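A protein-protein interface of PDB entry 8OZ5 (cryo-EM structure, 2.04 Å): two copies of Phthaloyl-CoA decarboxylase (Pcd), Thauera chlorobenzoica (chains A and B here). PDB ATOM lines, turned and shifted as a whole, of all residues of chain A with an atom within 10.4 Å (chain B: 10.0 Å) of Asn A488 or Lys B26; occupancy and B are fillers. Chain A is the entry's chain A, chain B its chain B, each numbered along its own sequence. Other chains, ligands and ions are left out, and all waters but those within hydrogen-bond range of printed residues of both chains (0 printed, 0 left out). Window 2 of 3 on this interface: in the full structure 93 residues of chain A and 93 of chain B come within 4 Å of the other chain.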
ATOM      1  N   ASP A 482      -8.323 -16.405   5.762  1.00  0.00           N
ATOM      2  CA  ASP A 482      -8.800 -15.599   6.874  1.00  0.00           C
ATOM      3  C   ASP A 482      -8.204 -14.200   6.874  1.00  0.00           C
ATOM      4  O   ASP A 482      -8.635 -13.356   7.665  1.00  0.00           O
ATOM      5  CB  ASP A 482      -8.479 -16.295   8.198  1.00  0.00           C
ATOM      6  CG  ASP A 482      -7.002 -16.581   8.356  1.00  0.00           C
ATOM      7  OD1 ASP A 482      -6.330 -16.807   7.327  1.00  0.00           O
ATOM      8  OD2 ASP A 482      -6.511 -16.579   9.504  1.00  0.00           O
ATOM      9  N   LEU A 483      -7.228 -13.938   6.010  1.00  0.00           N
ATOM     10  CA  LEU A 483      -6.520 -12.668   5.971  1.00  0.00           C
ATOM     11  C   LEU A 483      -7.123 -11.681   4.984  1.00  0.00           C
ATOM     12  O   LEU A 483      -6.688 -10.527   4.938  1.00  0.00           O
ATOM     13  CB  LEU A 483      -5.049 -12.903   5.624  1.00  0.00           C
ATOM     14  CG  LEU A 483      -4.265 -13.727   6.645  1.00  0.00           C
ATOM     15  CD1 LEU A 483      -3.127 -14.473   5.978  1.00  0.00           C
ATOM     16  CD2 LEU A 483      -3.736 -12.835   7.749  1.00  0.00           C
ATOM     17  N   VAL A 484      -8.104 -12.103   4.192  1.00  0.00           N
ATOM     18  CA  VAL A 484      -8.717 -11.253   3.181  1.00  0.00           C
ATOM     19  C   VAL A 484     -10.223 -11.438   3.248  1.00  0.00           C
ATOM     20  O   VAL A 484     -10.714 -12.539   3.515  1.00  0.00           O
ATOM     21  CB  VAL A 484      -8.178 -11.573   1.772  1.00  0.00           C
ATOM     22  CG1 VAL A 484      -8.583 -12.975   1.352  1.00  0.00           C
ATOM     23  CG2 VAL A 484      -8.679 -10.554   0.771  1.00  0.00           C
ATOM     24  N   LYS A 485     -10.957 -10.355   3.019  1.00  0.00           N
ATOM     25  CA  LYS A 485     -12.405 -10.387   3.100  1.00  0.00           C
ATOM     26  C   LYS A 485     -13.010 -10.123   1.733  1.00  0.00           C
ATOM     27  O   LYS A 485     -12.761  -9.059   1.151  1.00  0.00           O
ATOM     28  CB  LYS A 485     -12.908  -9.348   4.106  1.00  0.00           C
ATOM     29  CG  LYS A 485     -12.507  -9.642   5.541  1.00  0.00           C
ATOM     30  CD  LYS A 485     -13.063  -8.602   6.498  1.00  0.00           C
ATOM     31  CE  LYS A 485     -12.818  -8.998   7.949  1.00  0.00           C
ATOM     32  NZ  LYS A 485     -11.374  -9.013   8.322  1.00  0.00           N
ATOM     33  N   PRO A 486     -13.807 -11.048   1.196  1.00  0.00           N
ATOM     34  CA  PRO A 486     -14.341 -10.855  -0.161  1.00  0.00           C
ATOM     35  C   PRO A 486     -15.256  -9.652  -0.289  1.00  0.00           C
ATOM     36  O   PRO A 486     -15.436  -9.141  -1.401  1.00  0.00           O
ATOM     37  CB  PRO A 486     -15.099 -12.163  -0.430  1.00  0.00           C
ATOM     38  CG  PRO A 486     -14.588 -13.134   0.588  1.00  0.00           C
ATOM     39  CD  PRO A 486     -14.253 -12.318   1.789  1.00  0.00           C
ATOM     40  N   GLU A 487     -15.850  -9.184   0.812  1.00  0.00           N
ATOM     41  CA  GLU A 487     -16.729  -8.022   0.738  1.00  0.00           C
ATOM     42  C   GLU A 487     -15.959  -6.765   0.356  1.00  0.00           C
ATOM     43  O   GLU A 487     -16.533  -5.840  -0.228  1.00  0.00           O
ATOM     44  CB  GLU A 487     -17.503  -7.762   2.052  1.00  0.00           C
ATOM     45  CG  GLU A 487     -18.039  -8.891   3.014  1.00  0.00           C
ATOM     46  CD  GLU A 487     -17.152 -10.097   3.276  1.00  0.00           C
ATOM     47  OE1 GLU A 487     -15.989 -10.095   2.828  1.00  0.00           O
ATOM     48  OE2 GLU A 487     -17.617 -11.043   3.946  1.00  0.00           O
ATOM     49  N   ASN A 488     -14.666  -6.709   0.673  1.00  0.00           N
ATOM     50  CA  ASN A 488     -13.879  -5.534   0.323  1.00  0.00           C
ATOM     51  C   ASN A 488     -13.630  -5.446  -1.175  1.00  0.00           C
ATOM     52  O   ASN A 488     -13.306  -4.367  -1.684  1.00  0.00           O
ATOM     53  CB  ASN A 488     -12.551  -5.550   1.074  1.00  0.00           C
ATOM     54  CG  ASN A 488     -12.733  -5.483   2.574  1.00  0.00           C
ATOM     55  OD1 ASN A 488     -13.774  -5.049   3.068  1.00  0.00           O
ATOM     56  ND2 ASN A 488     -11.721  -5.921   3.310  1.00  0.00           N
ATOM     57  N   PHE A 489     -13.768  -6.558  -1.893  1.00  0.00           N
ATOM     58  CA  PHE A 489     -13.437  -6.612  -3.311  1.00  0.00           C
ATOM     59  C   PHE A 489     -14.656  -6.744  -4.211  1.00  0.00           C
ATOM     60  O   PHE A 489     -14.721  -6.086  -5.252  1.00  0.00           O
ATOM     61  CB  PHE A 489     -12.477  -7.772  -3.581  1.00  0.00           C
ATOM     62  CG  PHE A 489     -11.136  -7.605  -2.935  1.00  0.00           C
ATOM     63  CD1 PHE A 489     -10.923  -8.015  -1.633  1.00  0.00           C
ATOM     64  CD2 PHE A 489     -10.090  -7.023  -3.628  1.00  0.00           C
ATOM     65  CE1 PHE A 489      -9.690  -7.857  -1.037  1.00  0.00           C
ATOM     66  CE2 PHE A 489      -8.856  -6.861  -3.037  1.00  0.00           C
ATOM     67  CZ  PHE A 489      -8.656  -7.279  -1.740  1.00  0.00           C
ATOM     68  N   PHE A 490     -15.622  -7.574  -3.838  1.00  0.00           N
ATOM     69  CA  PHE A 490     -16.812  -7.798  -4.642  1.00  0.00           C
ATOM     70  C   PHE A 490     -18.058  -7.482  -3.827  1.00  0.00           C
ATOM     71  O   PHE A 490     -18.018  -7.360  -2.601  1.00  0.00           O
ATOM     72  CB  PHE A 490     -16.872  -9.243  -5.152  1.00  0.00           C
ATOM     73  CG  PHE A 490     -15.544  -9.789  -5.577  1.00  0.00           C
ATOM     74  CD1 PHE A 490     -15.001  -9.451  -6.803  1.00  0.00           C
ATOM     75  CD2 PHE A 490     -14.837 -10.645  -4.752  1.00  0.00           C
ATOM     76  CE1 PHE A 490     -13.780  -9.954  -7.196  1.00  0.00           C
ATOM     77  CE2 PHE A 490     -13.615 -11.149  -5.140  1.00  0.00           C
ATOM     78  CZ  PHE A 490     -13.085 -10.804  -6.364  1.00  0.00           C
ATOM     79  N   ASP A 491     -19.176  -7.349  -4.531  1.00  0.00           N
ATOM     80  CA  ASP A 491     -20.473  -7.154  -3.906  1.00  0.00           C
ATOM     81  C   ASP A 491     -21.088  -8.503  -3.551  1.00  0.00           C
ATOM     82  O   ASP A 491     -20.568  -9.563  -3.900  1.00  0.00           O
ATOM     83  CB  ASP A 491     -21.401  -6.362  -4.828  1.00  0.00           C
ATOM     84  CG  ASP A 491     -21.439  -6.923  -6.228  1.00  0.00           C
ATOM     85  OD1 ASP A 491     -20.649  -7.844  -6.521  1.00  0.00           O
ATOM     86  OD2 ASP A 491     -22.257  -6.442  -7.038  1.00  0.00           O
ATOM     87  N   ALA A 492     -22.214  -8.448  -2.837  1.00  0.00           N
ATOM     88  CA  ALA A 492     -22.832  -9.669  -2.331  1.00  0.00           C
ATOM     89  C   ALA A 492     -23.318 -10.557  -3.469  1.00  0.00           C
ATOM     90  O   ALA A 492     -23.287 -11.788  -3.373  1.00  0.00           O
ATOM     91  CB  ALA A 492     -23.986  -9.317  -1.393  1.00  0.00           C
ATOM     92  N   ILE A 495     -20.431 -12.554  -4.986  1.00  0.00           N
ATOM     93  CA  ILE A 495     -19.970 -13.520  -3.995  1.00  0.00           C
ATOM     94  C   ILE A 495     -20.924 -14.702  -3.928  1.00  0.00           C
ATOM     95  O   ILE A 495     -20.494 -15.860  -3.868  1.00  0.00           O
ATOM     96  CB  ILE A 495     -19.802 -12.847  -2.622  1.00  0.00           C
ATOM     97  CG1 ILE A 495     -18.681 -11.809  -2.671  1.00  0.00           C
ATOM     98  CG2 ILE A 495     -19.502 -13.885  -1.558  1.00  0.00           C
ATOM     99  CD1 ILE A 495     -18.374 -11.188  -1.330  1.00  0.00           C
ATOM    100  N   VAL B  22     -16.221 -12.059 -13.120  1.00  0.00           N
ATOM    101  CA  VAL B  22     -16.393 -11.249 -11.921  1.00  0.00           C
ATOM    102  C   VAL B  22     -15.245 -10.252 -11.869  1.00  0.00           C
ATOM    103  O   VAL B  22     -14.082 -10.646 -11.722  1.00  0.00           O
ATOM    104  CB  VAL B  22     -16.431 -12.110 -10.650  1.00  0.00           C
ATOM    105  CG1 VAL B  22     -16.396 -11.231  -9.418  1.00  0.00           C
ATOM    106  CG2 VAL B  22     -17.669 -12.985 -10.646  1.00  0.00           C
ATOM    107  N   GLU B  23     -15.569  -8.971 -11.989  1.00  0.00           N
ATOM    108  CA  GLU B  23     -14.579  -7.906 -12.012  1.00  0.00           C
ATOM    109  C   GLU B  23     -14.586  -7.141 -10.697  1.00  0.00           C
ATOM    110  O   GLU B  23     -15.545  -7.183  -9.923  1.00  0.00           O
ATOM    111  CB  GLU B  23     -14.837  -6.944 -13.174  1.00  0.00           C
ATOM    112  CG  GLU B  23     -14.790  -7.584 -14.541  1.00  0.00           C
ATOM    113  CD  GLU B  23     -14.574  -6.567 -15.641  1.00  0.00           C
ATOM    114  OE1 GLU B  23     -13.776  -5.629 -15.434  1.00  0.00           O
ATOM    115  OE2 GLU B  23     -15.203  -6.703 -16.709  1.00  0.00           O
ATOM    116  N   THR B  24     -13.490  -6.430 -10.456  1.00  0.00           N
ATOM    117  CA  THR B  24     -13.378  -5.560  -9.296  1.00  0.00           C
ATOM    118  C   THR B  24     -12.278  -4.546  -9.560  1.00  0.00           C
ATOM    119  O   THR B  24     -11.267  -4.861 -10.192  1.00  0.00           O
ATOM    120  CB  THR B  24     -13.083  -6.348  -8.017  1.00  0.00           C
ATOM    121  OG1 THR B  24     -13.135  -5.467  -6.888  1.00  0.00           O
ATOM    122  CG2 THR B  24     -11.707  -6.982  -8.089  1.00  0.00           C
ATOM    123  N   ASN B  25     -12.489  -3.328  -9.071  1.00  0.00           N
ATOM    124  CA  ASN B  25     -11.517  -2.255  -9.216  1.00  0.00           C
ATOM    125  C   ASN B  25     -10.725  -2.001  -7.944  1.00  0.00           C
ATOM    126  O   ASN B  25      -9.781  -1.207  -7.969  1.00  0.00           O
ATOM    127  CB  ASN B  25     -12.212  -0.964  -9.659  1.00  0.00           C
ATOM    128  CG  ASN B  25     -12.633  -1.001 -11.112  1.00  0.00           C
ATOM    129  OD1 ASN B  25     -11.886  -1.461 -11.975  1.00  0.00           O
ATOM    130  ND2 ASN B  25     -13.835  -0.515 -11.392  1.00  0.00           N
ATOM    131  N   LYS B  26     -11.084  -2.646  -6.838  1.00  0.00           N
ATOM    132  CA  LYS B  26     -10.314  -2.511  -5.613  1.00  0.00           C
ATOM    133  C   LYS B  26      -8.910  -3.061  -5.817  1.00  0.00           C
ATOM    134  O   LYS B  26      -8.720  -4.108  -6.442  1.00  0.00           O
ATOM    135  CB  LYS B  26     -11.004  -3.244  -4.465  1.00  0.00           C
ATOM    136  CG  LYS B  26     -12.460  -2.870  -4.282  1.00  0.00           C
ATOM    137  CD  LYS B  26     -12.620  -1.384  -4.027  1.00  0.00           C
ATOM    138  CE  LYS B  26     -13.986  -1.073  -3.445  1.00  0.00           C
ATOM    139  NZ  LYS B  26     -15.080  -1.697  -4.239  1.00  0.00           N
ATOM    140  N   GLU B  27      -7.922  -2.348  -5.288  1.00  0.00           N
ATOM    141  CA  GLU B  27      -6.537  -2.768  -5.449  1.00  0.00           C
ATOM    142  C   GLU B  27      -6.281  -4.047  -4.666  1.00  0.00           C
ATOM    143  O   GLU B  27      -6.468  -4.091  -3.446  1.00  0.00           O
ATOM    144  CB  GLU B  27      -5.589  -1.666  -4.984  1.00  0.00           C
ATOM    145  CG  GLU B  27      -4.172  -1.814  -5.508  1.00  0.00           C
ATOM    146  CD  GLU B  27      -3.150  -1.152  -4.609  1.00  0.00           C
ATOM    147  OE1 GLU B  27      -3.217  -1.359  -3.379  1.00  0.00           O
ATOM    148  OE2 GLU B  27      -2.279  -0.425  -5.131  1.00  0.00           O
ATOM    149  N   VAL B  28      -5.853  -5.088  -5.367  1.00  0.00           N
ATOM    150  CA  VAL B  28      -5.531  -6.369  -4.752  1.00  0.00           C
ATOM    151  C   VAL B  28      -4.029  -6.432  -4.532  1.00  0.00           C
ATOM    152  O   VAL B  28      -3.242  -5.989  -5.377  1.00  0.00           O
ATOM    153  CB  VAL B  28      -6.015  -7.545  -5.618  1.00  0.00           C
ATOM    154  CG1 VAL B  28      -5.220  -7.620  -6.907  1.00  0.00           C
ATOM    155  CG2 VAL B  28      -5.905  -8.848  -4.844  1.00  0.00           C
ATOM    156  N   ASN B  29      -3.629  -6.981  -3.390  1.00  0.00           N
ATOM    157  CA  ASN B  29      -2.220  -7.093  -3.058  1.00  0.00           C
ATOM    158  C   ASN B  29      -1.705  -8.430  -3.560  1.00  0.00           C
ATOM    159  O   ASN B  29      -2.278  -9.472  -3.211  1.00  0.00           O
ATOM    160  CB  ASN B  29      -2.013  -6.971  -1.550  1.00  0.00           C
ATOM    161  CG  ASN B  29      -0.553  -6.859  -1.170  1.00  0.00           C
ATOM    162  OD1 ASN B  29       0.326  -6.850  -2.029  1.00  0.00           O
ATOM    163  ND2 ASN B  29      -0.287  -6.765   0.126  1.00  0.00           N
ATOM    164  N   PRO B  30      -0.642  -8.463  -4.366  1.00  0.00           N
ATOM    165  CA  PRO B  30      -0.106  -9.750  -4.832  1.00  0.00           C
ATOM    166  C   PRO B  30       0.434 -10.613  -3.703  1.00  0.00           C
ATOM    167  O   PRO B  30       0.657 -11.815  -3.881  1.00  0.00           O
ATOM    168  CB  PRO B  30       1.012  -9.331  -5.796  1.00  0.00           C
ATOM    169  CG  PRO B  30       0.662  -7.938  -6.204  1.00  0.00           C
ATOM    170  CD  PRO B  30       0.039  -7.321  -4.995  1.00  0.00           C
ATOM    171  N   GLU B  33      -3.023 -12.013  -1.079  1.00  0.00           N
ATOM    172  CA  GLU B  33      -4.421 -11.648  -1.285  1.00  0.00           C
ATOM    173  C   GLU B  33      -5.002 -12.321  -2.521  1.00  0.00           C
ATOM    174  O   GLU B  33      -6.148 -12.785  -2.499  1.00  0.00           O
ATOM    175  CB  GLU B  33      -4.562 -10.131  -1.383  1.00  0.00           C
ATOM    176  CG  GLU B  33      -4.656  -9.444  -0.035  1.00  0.00           C
ATOM    177  CD  GLU B  33      -5.151  -8.018  -0.142  1.00  0.00           C
ATOM    178  OE1 GLU B  33      -5.219  -7.492  -1.273  1.00  0.00           O
ATOM    179  OE2 GLU B  33      -5.473  -7.423   0.906  1.00  0.00           O
ATOM    180  N   ILE B  34      -4.234 -12.387  -3.608  1.00  0.00           N
ATOM    181  CA  ILE B  34      -4.739 -13.023  -4.822  1.00  0.00           C
ATOM    182  C   ILE B  34      -4.971 -14.509  -4.585  1.00  0.00           C
ATOM    183  O   ILE B  34      -6.050 -15.039  -4.878  1.00  0.00           O
ATOM    184  CB  ILE B  34      -3.776 -12.780  -5.997  1.00  0.00           C
ATOM    185  CG1 ILE B  34      -3.868 -11.331  -6.469  1.00  0.00           C
ATOM    186  CG2 ILE B  34      -4.085 -13.731  -7.139  1.00  0.00           C
ATOM    187  CD1 ILE B  34      -2.916 -10.997  -7.589  1.00  0.00           C
ATOM    188  N   LEU B  37      -7.931 -15.038  -2.113  1.00  0.00           N
ATOM    189  CA  LEU B  37      -9.242 -14.925  -2.742  1.00  0.00           C
ATOM    190  C   LEU B  37      -9.505 -16.096  -3.677  1.00  0.00           C
ATOM    191  O   LEU B  37     -10.646 -16.555  -3.799  1.00  0.00           O
ATOM    192  CB  LEU B  37      -9.351 -13.603  -3.497  1.00  0.00           C
ATOM    193  CG  LEU B  37      -9.619 -12.367  -2.642  1.00  0.00           C
ATOM    194  CD1 LEU B  37      -9.601 -11.117  -3.499  1.00  0.00           C
ATOM    195  CD2 LEU B  37     -10.942 -12.503  -1.919  1.00  0.00           C
ATOM    196  N   ILE B  40     -10.507 -18.940  -1.455  1.00  0.00           N
ATOM    197  CA  ILE B  40     -11.831 -18.738  -0.877  1.00  0.00           C
ATOM    198  C   ILE B  40     -12.915 -19.134  -1.868  1.00  0.00           C
ATOM    199  O   ILE B  40     -13.989 -19.601  -1.472  1.00  0.00           O
ATOM    200  CB  ILE B  40     -11.998 -17.279  -0.415  1.00  0.00           C
ATOM    201  CG1 ILE B  40     -11.268 -17.054   0.908  1.00  0.00           C
ATOM    202  CG2 ILE B  40     -13.466 -16.930  -0.272  1.00  0.00           C
ATOM    203  CD1 ILE B  40     -11.369 -15.638   1.417  1.00  0.00           C
ATOM    204  N   PHE B  41     -12.657 -18.963  -3.160  1.00  0.00           N
ATOM    205  CA  PHE B  41     -13.589 -19.332  -4.217  1.00  0.00           C
ATOM    206  C   PHE B  41     -13.004 -20.421  -5.109  1.00  0.00           C
ATOM    207  O   PHE B  41     -13.081 -20.347  -6.337  1.00  0.00           O
ATOM    208  CB  PHE B  41     -13.975 -18.112  -5.047  1.00  0.00           C
ATOM    209  CG  PHE B  41     -14.592 -17.009  -4.245  1.00  0.00           C
ATOM    210  CD1 PHE B  41     -15.901 -17.102  -3.812  1.00  0.00           C
ATOM    211  CD2 PHE B  41     -13.865 -15.878  -3.923  1.00  0.00           C
ATOM    212  CE1 PHE B  41     -16.473 -16.089  -3.075  1.00  0.00           C
ATOM    213  CE2 PHE B  41     -14.433 -14.862  -3.186  1.00  0.00           C
ATOM    214  CZ  PHE B  41     -15.739 -14.969  -2.761  1.00  0.00           C
ATOM    215  N   LEU B  48     -11.323 -11.121 -12.301  1.00  0.00           N
ATOM    216  CA  LEU B  48     -10.448 -10.172 -12.977  1.00  0.00           C
ATOM    217  C   LEU B  48     -10.199  -8.989 -12.055  1.00  0.00           C
ATOM    218  O   LEU B  48     -11.138  -8.278 -11.687  1.00  0.00           O
ATOM    219  CB  LEU B  48     -11.058  -9.703 -14.298  1.00  0.00           C
ATOM    220  CG  LEU B  48     -10.296  -8.601 -15.031  1.00  0.00           C
ATOM    221  CD1 LEU B  48      -8.880  -9.046 -15.331  1.00  0.00           C
ATOM    222  CD2 LEU B  48     -11.015  -8.214 -16.307  1.00  0.00           C
ATOM    223  N   PHE B  49      -8.939  -8.781 -11.690  1.00  0.00           N
ATOM    224  CA  PHE B  49      -8.537  -7.660 -10.852  1.00  0.00           C
ATOM    225  C   PHE B  49      -7.931  -6.579 -11.736  1.00  0.00           C
ATOM    226  O   PHE B  49      -6.862  -6.779 -12.321  1.00  0.00           O
ATOM    227  CB  PHE B  49      -7.539  -8.107  -9.785  1.00  0.00           C
ATOM    228  CG  PHE B  49      -8.082  -9.140  -8.845  1.00  0.00           C
ATOM    229  CD1 PHE B  49      -8.826  -8.766  -7.743  1.00  0.00           C
ATOM    230  CD2 PHE B  49      -7.844 -10.485  -9.062  1.00  0.00           C
ATOM    231  CE1 PHE B  49      -9.325  -9.713  -6.875  1.00  0.00           C
ATOM    232  CE2 PHE B  49      -8.341 -11.436  -8.197  1.00  0.00           C
ATOM    233  CZ  PHE B  49      -9.083 -11.050  -7.102  1.00  0.00           C
ATOM    234  N   ASN B  50      -8.614  -5.439 -11.831  1.00  0.00           N
ATOM    235  CA  ASN B  50      -8.160  -4.363 -12.699  1.00  0.00           C
ATOM    236  C   ASN B  50      -7.012  -3.562 -12.102  1.00  0.00           C
ATOM    237  O   ASN B  50      -6.253  -2.944 -12.854  1.00  0.00           O
ATOM    238  CB  ASN B  50      -9.322  -3.423 -13.023  1.00  0.00           C
ATOM    239  CG  ASN B  50     -10.260  -3.997 -14.063  1.00  0.00           C
ATOM    240  OD1 ASN B  50      -9.827  -4.472 -15.111  1.00  0.00           O
ATOM    241  ND2 ASN B  50     -11.554  -3.955 -13.779  1.00  0.00           N
ATOM    242  N   ASN B  51      -6.862  -3.560 -10.781  1.00  0.00           N
ATOM    243  CA  ASN B  51      -5.826  -2.786 -10.107  1.00  0.00           C
ATOM    244  C   ASN B  51      -5.010  -3.713  -9.219  1.00  0.00           C
ATOM    245  O   ASN B  51      -5.540  -4.287  -8.262  1.00  0.00           O
ATOM    246  CB  ASN B  51      -6.437  -1.652  -9.285  1.00  0.00           C
ATOM    247  CG  ASN B  51      -7.263  -0.707 -10.128  1.00  0.00           C
ATOM    248  OD1 ASN B  51      -6.823  -0.252 -11.182  1.00  0.00           O
ATOM    249  ND2 ASN B  51      -8.470  -0.407  -9.668  1.00  0.00           N
ATOM    250  N   VAL B  52      -3.725  -3.848  -9.532  1.00  0.00           N
ATOM    251  CA  VAL B  52      -2.798  -4.670  -8.765  1.00  0.00           C
ATOM    252  C   VAL B  52      -1.835  -3.748  -8.036  1.00  0.00           C
ATOM    253  O   VAL B  52      -1.291  -2.811  -8.633  1.00  0.00           O
ATOM    254  CB  VAL B  52      -2.040  -5.658  -9.665  1.00  0.00           C
ATOM    255  CG1 VAL B  52      -1.187  -6.590  -8.822  1.00  0.00           C
ATOM    256  CG2 VAL B  52      -3.014  -6.445 -10.518  1.00  0.00           C
ATOM    257  N   LYS B  53      -1.626  -4.012  -6.749  1.00  0.00           N
ATOM    258  CA  LYS B  53      -0.786  -3.150  -5.930  1.00  0.00           C
ATOM    259  C   LYS B  53       0.650  -3.149  -6.436  1.00  0.00           C
ATOM    260  O   LYS B  53       1.255  -4.207  -6.630  1.00  0.00           O
ATOM    261  CB  LYS B  53      -0.831  -3.605  -4.473  1.00  0.00           C
ATOM    262  CG  LYS B  53       0.047  -2.786  -3.545  1.00  0.00           C
ATOM    263  CD  LYS B  53      -0.269  -3.082  -2.092  1.00  0.00           C
ATOM    264  CE  LYS B  53       0.667  -2.334  -1.160  1.00  0.00           C
ATOM    265  NZ  LYS B  53       2.033  -2.920  -1.164  1.00  0.00           N
ATOM    266  N   ALA B  58      -0.537  -3.495 -15.003  1.00  0.00           N
ATOM    267  CA  ALA B  58      -0.916  -4.893 -15.121  1.00  0.00           C
ATOM    268  C   ALA B  58      -2.317  -5.134 -14.580  1.00  0.00           C
ATOM    269  O   ALA B  58      -2.744  -4.513 -13.603  1.00  0.00           O
ATOM    270  CB  ALA B  58       0.077  -5.795 -14.380  1.00  0.00           C
ATOM    271  N   ARG B  59      -3.026  -6.048 -15.234  1.00  0.00           N
ATOM    272  CA  ARG B  59      -4.263  -6.613 -14.724  1.00  0.00           C
ATOM    273  C   ARG B  59      -4.031  -8.084 -14.413  1.00  0.00           C
ATOM    274  O   ARG B  59      -3.238  -8.754 -15.079  1.00  0.00           O
ATOM    275  CB  ARG B  59      -5.412  -6.467 -15.725  1.00  0.00           C
ATOM    276  CG  ARG B  59      -5.791  -5.035 -16.042  1.00  0.00           C
ATOM    277  CD  ARG B  59      -7.165  -4.965 -16.681  1.00  0.00           C
ATOM    278  NE  ARG B  59      -7.235  -5.735 -17.919  1.00  0.00           N
ATOM    279  CZ  ARG B  59      -6.980  -5.238 -19.124  1.00  0.00           C
ATOM    280  NH1 ARG B  59      -6.639  -3.965 -19.258  1.00  0.00           N
ATOM    281  NH2 ARG B  59      -7.070  -6.012 -20.195  1.00  0.00           N
ATOM    282  N   ALA B  60      -4.724  -8.583 -13.397  1.00  0.00           N
ATOM    283  CA  ALA B  60      -4.552  -9.957 -12.957  1.00  0.00           C
ATOM    284  C   ALA B  60      -5.882 -10.688 -13.013  1.00  0.00           C
ATOM    285  O   ALA B  60      -6.891 -10.204 -12.494  1.00  0.00           O
ATOM    286  CB  ALA B  60      -3.981 -10.023 -11.537  1.00  0.00           C
ATOM    287  N   LYS B 311      -2.862  -2.184 -20.396  1.00  0.00           N
ATOM    288  CA  LYS B 311      -2.786  -2.976 -19.175  1.00  0.00           C
ATOM    289  C   LYS B 311      -2.817  -4.469 -19.486  1.00  0.00           C
ATOM    290  O   LYS B 311      -3.852  -5.119 -19.292  1.00  0.00           O
ATOM    291  CB  LYS B 311      -3.923  -2.603 -18.224  1.00  0.00           C
ATOM    292  CG  LYS B 311      -3.751  -1.238 -17.577  1.00  0.00           C
ATOM    293  CD  LYS B 311      -5.021  -0.790 -16.876  1.00  0.00           C
ATOM    294  CE  LYS B 311      -5.171  -1.464 -15.524  1.00  0.00           C
ATOM    295  NZ  LYS B 311      -4.170  -0.965 -14.544  1.00  0.00           N
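The backbone carbonyl oxygen (O) of Phe A489 lies close to the side-chain hydroxyl (OG1) of Thr B24.
No position is printed for both chains.
Along chain A the printed residues that touch a printed residue of chain B span positions 484 to 490.
Printed residues of chain B that touch a printed residue of chain A: Val B22, Glu B23, Thr B24, Lys B26, Glu B27, Val B28, Glu B33, Leu B37, Ile B40, Phe B41 and Phe B49.
Among the printed residues, 14 pairs touch across the chains.
Among the printed residues, no Asp or Glu carboxylate lies within 4 Å of a Lys or Arg side-chain nitrogen of the other chain.
No residue of chain B comes within 4 Å of Lys A485.
Asn A488 touches one residue of chain B.
Phe A489 touches just these residues of chain B: Thr B24 (2.4 Å), Lys B26 (3.98 Å), Glu B27 (3.7 Å), Val B28 (3.8 Å), Glu B33 (3.5 Å) and Leu B37 (3.9 Å).
Of the printed residues of chain B, Phe A490 touches Val B22 (3.5 Å), Glu B23 (3.9 Å), Thr B24 (3.7 Å) and Phe B49 (3.9 Å).
No residue of chain A comes within 4 Å of Asn B25.
Of chain A, only Asn A488 and Phe A489 come within 4 Å of Lys B26.
Printed residues of chain A within 4 Å of Glu B27: Phe A489.
Of chain A, only Phe A489 (3.8 Å) comes within 4 Å of Val B28.
Of the printed residues of chain A, Ile B40 touches Val A484 (3.8 Å).
Of the printed residues of chain A, Phe B49 touches Phe A490 (3.9 Å).
The nearest printed residue of chain A that does not touch Glu B23 is Phe A489 (4.9 Å).
Val A484 touches Leu B37.
Asn A488 touches Lys B26.
Phe A489 touches Glu B27.
Phe A489 touches Val B28 (CE2 to CA, 3.8 Å).
OE1 of Glu B33 touches CZ of Phe A489, at 3.5 Å.
Phe A489 touches Leu B37 (CD1 to CD1, 3.9 Å).
CD1 of Phe A490 touches CG1 of Val B22, at 3.5 Å.
Phe A490 touches Glu B23.
Thr B24 touches Phe A490 (CG2 to CE1, 3.7 Å).
Phe A490 touches Phe B49 (CZ to CE1, 3.9 Å).
The backbone carbonyl oxygen (O) of Val B22 lies within hydrogen-bond range of the backbone NH (N) of Leu B48.
The side-chain carboxylate (OE1) of Glu B23 sits at hydrogen-bond distance from the side-chain amide nitrogen (ND2) of Asn B50.
O of Leu B48 lies within hydrogen-bond range of N of Thr B24 (3.2 Å).
The backbone NH (N) of Asn B50 sits at hydrogen-bond distance from the backbone carbonyl oxygen (O) of Thr B24 (3.2 Å).
N of Lys B53 lies within hydrogen-bond range of O of Val B28, at 2.9 Å.
The backbone NH (N) of Phe B49 lies within hydrogen-bond range of the backbone carbonyl oxygen (O) of Ala B60.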
